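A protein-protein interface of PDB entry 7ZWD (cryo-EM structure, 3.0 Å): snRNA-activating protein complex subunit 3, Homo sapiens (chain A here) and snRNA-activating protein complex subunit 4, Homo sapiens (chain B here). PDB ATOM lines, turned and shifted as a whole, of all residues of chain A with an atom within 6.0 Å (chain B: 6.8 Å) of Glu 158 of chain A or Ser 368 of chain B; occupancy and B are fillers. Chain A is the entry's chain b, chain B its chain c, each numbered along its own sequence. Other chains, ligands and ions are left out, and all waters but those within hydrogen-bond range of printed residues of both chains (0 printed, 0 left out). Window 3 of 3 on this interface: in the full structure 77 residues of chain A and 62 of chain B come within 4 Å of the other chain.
The side-chain hydroxyl of Ser 368 of chain B lies within hydrogen-bond range of the side-chain carboxylate of Glu 158 of chain A, 2.8 Å away. The backbone carbonyl oxygen (O) of Glu 158 of chain A lies close to the backbone carbonyl oxygen (O) of Val 366 of chain B (3.2 Å).
NH2 of Arg 365 of chain B sits at hydrogen-bond distance from O of Gly 367 of chain B (2.6 Å).
CE1 of His 369 of chain B touches CD1 of Phe 155 of chain A (3.4 Å). Gly 367 of chain B touches Glu 158 of chain A. Met 159 of chain A touches Val 366 of chain B. His 162 of chain A touches Val 366 of chain B.
Glu 153 of chain A touches none of the printed residues of chain B. Tyr 157 of chain A touches none of the printed residues of chain B. Of chain B, only Val 366 (3.2 Å), Gly 367 (3.2 Å) and Ser 368 (2.8 Å) come within 4 Å of Glu 158 of chain A. Of the printed residues of chain B, Met 159 of chain A touches Val 366. Printed residues of chain B within 4 Å of His 162 of chain A: Val 366 (3.5 Å). Printed residues of chain A within 4 Å of Val 366 of chain B: Glu 158 (3.2 Å), Met 159 (3.9 Å) and His 162 (3.5 Å). Printed residues of chain A within 4 Å of Gly 367 of chain B: Glu 158. Ser 368 of chain B touches one residue of chain A. The nearest residue of chain A that does not touch Ser 368 of chain B is Thr 154 of chain A (4.6 Å). The nearest printed residue of chain A that does not touch Val 366 of chain B is Phe 155 of chain A (4.9 Å).
Hydrophobic or aromatic side chains of chain B within 4 Å of the printed part of chain A: Val 366 and His 369. Among the printed residues, no Asp or Glu carboxylate lies within 4 Å of a Lys or Arg side-chain nitrogen of the other chain.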
ATOM      1  N   GLU A 153      31.365  11.719 -29.070  1.00  0.00           N
ATOM      2  CA  GLU A 153      31.000  10.380 -28.631  1.00  0.00           C
ATOM      3  C   GLU A 153      29.559  10.339 -28.153  1.00  0.00           C
ATOM      4  O   GLU A 153      28.774   9.488 -28.589  1.00  0.00           O
ATOM      5  CB  GLU A 153      31.938   9.917 -27.522  1.00  0.00           C
ATOM      6  CG  GLU A 153      31.645   8.524 -27.014  1.00  0.00           C
ATOM      7  CD  GLU A 153      32.588   8.103 -25.912  1.00  0.00           C
ATOM      8  OE1 GLU A 153      33.445   8.917 -25.521  1.00  0.00           O
ATOM      9  OE2 GLU A 153      32.477   6.958 -25.438  1.00  0.00           O
ATOM     10  N   THR A 154      29.195  11.242 -27.240  1.00  0.00           N
ATOM     11  CA  THR A 154      27.820  11.284 -26.764  1.00  0.00           C
ATOM     12  C   THR A 154      26.864  11.566 -27.904  1.00  0.00           C
ATOM     13  O   THR A 154      25.753  11.038 -27.931  1.00  0.00           O
ATOM     14  CB  THR A 154      27.652  12.339 -25.683  1.00  0.00           C
ATOM     15  OG1 THR A 154      27.777  13.635 -26.271  1.00  0.00           O
ATOM     16  CG2 THR A 154      28.702  12.176 -24.622  1.00  0.00           C
ATOM     17  N   PHE A 155      27.278  12.391 -28.862  1.00  0.00           N
ATOM     18  CA  PHE A 155      26.405  12.690 -29.988  1.00  0.00           C
ATOM     19  C   PHE A 155      26.135  11.449 -30.821  1.00  0.00           C
ATOM     20  O   PHE A 155      24.979  11.117 -31.098  1.00  0.00           O
ATOM     21  CB  PHE A 155      27.023  13.776 -30.849  1.00  0.00           C
ATOM     22  CG  PHE A 155      26.360  13.938 -32.166  1.00  0.00           C
ATOM     23  CD1 PHE A 155      25.061  14.375 -32.243  1.00  0.00           C
ATOM     24  CD2 PHE A 155      27.037  13.662 -33.327  1.00  0.00           C
ATOM     25  CE1 PHE A 155      24.452  14.531 -33.454  1.00  0.00           C
ATOM     26  CE2 PHE A 155      26.429  13.814 -34.535  1.00  0.00           C
ATOM     27  CZ  PHE A 155      25.137  14.250 -34.598  1.00  0.00           C
ATOM     28  N   VAL A 156      27.193  10.749 -31.233  1.00  0.00           N
ATOM     29  CA  VAL A 156      27.020   9.556 -32.053  1.00  0.00           C
ATOM     30  C   VAL A 156      26.207   8.514 -31.308  1.00  0.00           C
ATOM     31  O   VAL A 156      25.329   7.862 -31.884  1.00  0.00           O
ATOM     32  CB  VAL A 156      28.384   8.996 -32.484  1.00  0.00           C
ATOM     33  CG1 VAL A 156      28.209   7.649 -33.118  1.00  0.00           C
ATOM     34  CG2 VAL A 156      29.046   9.931 -33.453  1.00  0.00           C
ATOM     35  N   TYR A 157      26.469   8.350 -30.013  1.00  0.00           N
ATOM     36  CA  TYR A 157      25.726   7.361 -29.246  1.00  0.00           C
ATOM     37  C   TYR A 157      24.255   7.735 -29.147  1.00  0.00           C
ATOM     38  O   TYR A 157      23.377   6.952 -29.522  1.00  0.00           O
ATOM     39  CB  TYR A 157      26.329   7.207 -27.859  1.00  0.00           C
ATOM     40  CG  TYR A 157      25.595   6.204 -27.026  1.00  0.00           C
ATOM     41  CD1 TYR A 157      25.589   4.870 -27.374  1.00  0.00           C
ATOM     42  CD2 TYR A 157      24.894   6.589 -25.903  1.00  0.00           C
ATOM     43  CE1 TYR A 157      24.920   3.945 -26.622  1.00  0.00           C
ATOM     44  CE2 TYR A 157      24.218   5.672 -25.145  1.00  0.00           C
ATOM     45  CZ  TYR A 157      24.234   4.349 -25.508  1.00  0.00           C
ATOM     46  OH  TYR A 157      23.562   3.420 -24.757  1.00  0.00           O
ATOM     47  N   GLU A 158      23.962   8.941 -28.658  1.00  0.00           N
ATOM     48  CA  GLU A 158      22.585   9.357 -28.466  1.00  0.00           C
ATOM     49  C   GLU A 158      21.827   9.481 -29.773  1.00  0.00           C
ATOM     50  O   GLU A 158      20.597   9.536 -29.751  1.00  0.00           O
ATOM     51  CB  GLU A 158      22.543  10.679 -27.715  1.00  0.00           C
ATOM     52  CG  GLU A 158      23.098  10.605 -26.311  1.00  0.00           C
ATOM     53  CD  GLU A 158      22.179   9.883 -25.350  1.00  0.00           C
ATOM     54  OE1 GLU A 158      21.002   9.665 -25.696  1.00  0.00           O
ATOM     55  OE2 GLU A 158      22.636   9.541 -24.242  1.00  0.00           O
ATOM     56  N   MET A 159      22.516   9.540 -30.907  1.00  0.00           N
ATOM     57  CA  MET A 159      21.797   9.438 -32.167  1.00  0.00           C
ATOM     58  C   MET A 159      21.523   7.986 -32.518  1.00  0.00           C
ATOM     59  O   MET A 159      20.409   7.640 -32.916  1.00  0.00           O
ATOM     60  CB  MET A 159      22.580  10.115 -33.283  1.00  0.00           C
ATOM     61  CG  MET A 159      22.474  11.610 -33.270  1.00  0.00           C
ATOM     62  SD  MET A 159      20.873  12.180 -33.827  1.00  0.00           S
ATOM     63  CE  MET A 159      20.863  11.515 -35.478  1.00  0.00           C
ATOM     64  N   GLU A 160      22.526   7.125 -32.367  1.00  0.00           N
ATOM     65  CA  GLU A 160      22.328   5.707 -32.630  1.00  0.00           C
ATOM     66  C   GLU A 160      21.250   5.123 -31.731  1.00  0.00           C
ATOM     67  O   GLU A 160      20.258   4.576 -32.220  1.00  0.00           O
ATOM     68  CB  GLU A 160      23.648   4.966 -32.448  1.00  0.00           C
ATOM     69  CG  GLU A 160      23.549   3.455 -32.388  1.00  0.00           C
ATOM     70  CD  GLU A 160      22.881   2.843 -33.596  1.00  0.00           C
ATOM     71  OE1 GLU A 160      21.640   2.724 -33.598  1.00  0.00           O
ATOM     72  OE2 GLU A 160      23.604   2.471 -34.543  1.00  0.00           O
ATOM     73  N   SER A 161      21.404   5.252 -30.413  1.00  0.00           N
ATOM     74  CA  SER A 161      20.463   4.673 -29.466  1.00  0.00           C
ATOM     75  C   SER A 161      19.298   5.595 -29.163  1.00  0.00           C
ATOM     76  O   SER A 161      18.704   5.502 -28.084  1.00  0.00           O
ATOM     77  CB  SER A 161      21.176   4.311 -28.169  1.00  0.00           C
ATOM     78  OG  SER A 161      21.522   5.479 -27.455  1.00  0.00           O
ATOM     79  N   HIS A 162      18.964   6.497 -30.080  1.00  0.00           N
ATOM     80  CA  HIS A 162      17.885   7.439 -29.823  1.00  0.00           C
ATOM     81  C   HIS A 162      16.550   6.729 -29.691  1.00  0.00           C
ATOM     82  O   HIS A 162      15.756   7.044 -28.799  1.00  0.00           O
ATOM     83  CB  HIS A 162      17.832   8.482 -30.934  1.00  0.00           C
ATOM     84  CG  HIS A 162      16.617   9.345 -30.891  1.00  0.00           C
ATOM     85  ND1 HIS A 162      15.547   9.162 -31.738  1.00  0.00           N
ATOM     86  CD2 HIS A 162      16.282  10.374 -30.077  1.00  0.00           C
ATOM     87  CE1 HIS A 162      14.615  10.056 -31.465  1.00  0.00           C
ATOM     88  NE2 HIS A 162      15.035  10.802 -30.459  1.00  0.00           N
ATOM     89  N   ALA A 163      16.288   5.757 -30.561  1.00  0.00           N
ATOM     90  CA  ALA A 163      15.011   5.051 -30.530  1.00  0.00           C
ATOM     91  C   ALA A 163      15.320   3.556 -30.631  1.00  0.00           C
ATOM     92  O   ALA A 163      15.416   3.009 -31.727  1.00  0.00           O
ATOM     93  CB  ALA A 163      14.092   5.500 -31.640  1.00  0.00           C
ATOM     94  N   ARG B 365      17.085  18.246 -28.201  1.00  0.00           N
ATOM     95  CA  ARG B 365      17.814  17.148 -27.590  1.00  0.00           C
ATOM     96  C   ARG B 365      17.683  15.918 -28.468  1.00  0.00           C
ATOM     97  O   ARG B 365      16.721  15.777 -29.225  1.00  0.00           O
ATOM     98  CB  ARG B 365      17.268  16.815 -26.208  1.00  0.00           C
ATOM     99  CG  ARG B 365      17.455  17.857 -25.153  1.00  0.00           C
ATOM    100  CD  ARG B 365      16.791  17.396 -23.878  1.00  0.00           C
ATOM    101  NE  ARG B 365      17.538  16.327 -23.241  1.00  0.00           N
ATOM    102  CZ  ARG B 365      18.389  16.517 -22.243  1.00  0.00           C
ATOM    103  NH1 ARG B 365      18.562  17.727 -21.745  1.00  0.00           N
ATOM    104  NH2 ARG B 365      19.040  15.492 -21.718  1.00  0.00           N
ATOM    105  N   VAL B 366      18.656  15.022 -28.366  1.00  0.00           N
ATOM    106  CA  VAL B 366      18.490  13.653 -28.821  1.00  0.00           C
ATOM    107  C   VAL B 366      18.746  12.672 -27.694  1.00  0.00           C
ATOM    108  O   VAL B 366      18.767  11.460 -27.919  1.00  0.00           O
ATOM    109  CB  VAL B 366      19.384  13.343 -30.025  1.00  0.00           C
ATOM    110  CG1 VAL B 366      19.233  14.411 -31.077  1.00  0.00           C
ATOM    111  CG2 VAL B 366      20.808  13.241 -29.583  1.00  0.00           C
ATOM    112  N   GLY B 367      18.910  13.172 -26.477  1.00  0.00           N
ATOM    113  CA  GLY B 367      19.299  12.369 -25.343  1.00  0.00           C
ATOM    114  C   GLY B 367      20.052  13.240 -24.367  1.00  0.00           C
ATOM    115  O   GLY B 367      19.537  14.266 -23.924  1.00  0.00           O
ATOM    116  N   SER B 368      21.263  12.844 -24.013  1.00  0.00           N
ATOM    117  CA  SER B 368      22.148  13.721 -23.270  1.00  0.00           C
ATOM    118  C   SER B 368      22.883  14.694 -24.174  1.00  0.00           C
ATOM    119  O   SER B 368      23.713  15.464 -23.687  1.00  0.00           O
ATOM    120  CB  SER B 368      23.156  12.898 -22.470  1.00  0.00           C
ATOM    121  OG  SER B 368      23.728  11.884 -23.276  1.00  0.00           O
ATOM    122  N   HIS B 369      22.602  14.672 -25.472  1.00  0.00           N
ATOM    123  CA  HIS B 369      23.233  15.558 -26.437  1.00  0.00           C
ATOM    124  C   HIS B 369      22.342  16.769 -26.656  1.00  0.00           C
ATOM    125  O   HIS B 369      21.272  16.653 -27.256  1.00  0.00           O
ATOM    126  CB  HIS B 369      23.506  14.877 -27.772  1.00  0.00           C
ATOM    127  CG  HIS B 369      23.752  15.831 -28.895  1.00  0.00           C
ATOM    128  ND1 HIS B 369      22.846  16.031 -29.910  1.00  0.00           N
ATOM    129  CD2 HIS B 369      24.803  16.639 -29.165  1.00  0.00           C
ATOM    130  CE1 HIS B 369      23.329  16.918 -30.760  1.00  0.00           C
ATOM    131  NE2 HIS B 369      24.515  17.303 -30.329  1.00  0.00           N
ATOM    132  N   ILE B 370      22.784  17.921 -26.174  1.00  0.00           N
ATOM    133  CA  ILE B 370      22.062  19.175 -26.307  1.00  0.00           C
ATOM    134  C   ILE B 370      22.911  20.097 -27.170  1.00  0.00           C
ATOM    135  O   ILE B 370      23.848  20.715 -26.665  1.00  0.00           O
ATOM    136  CB  ILE B 370      21.791  19.822 -24.942  1.00  0.00           C
ATOM    137  CG1 ILE B 370      21.214  18.795 -23.983  1.00  0.00           C
ATOM    138  CG2 ILE B 370      20.852  20.978 -25.093  1.00  0.00           C
ATOM    139  CD1 ILE B 370      21.370  19.177 -22.548  1.00  0.00           C
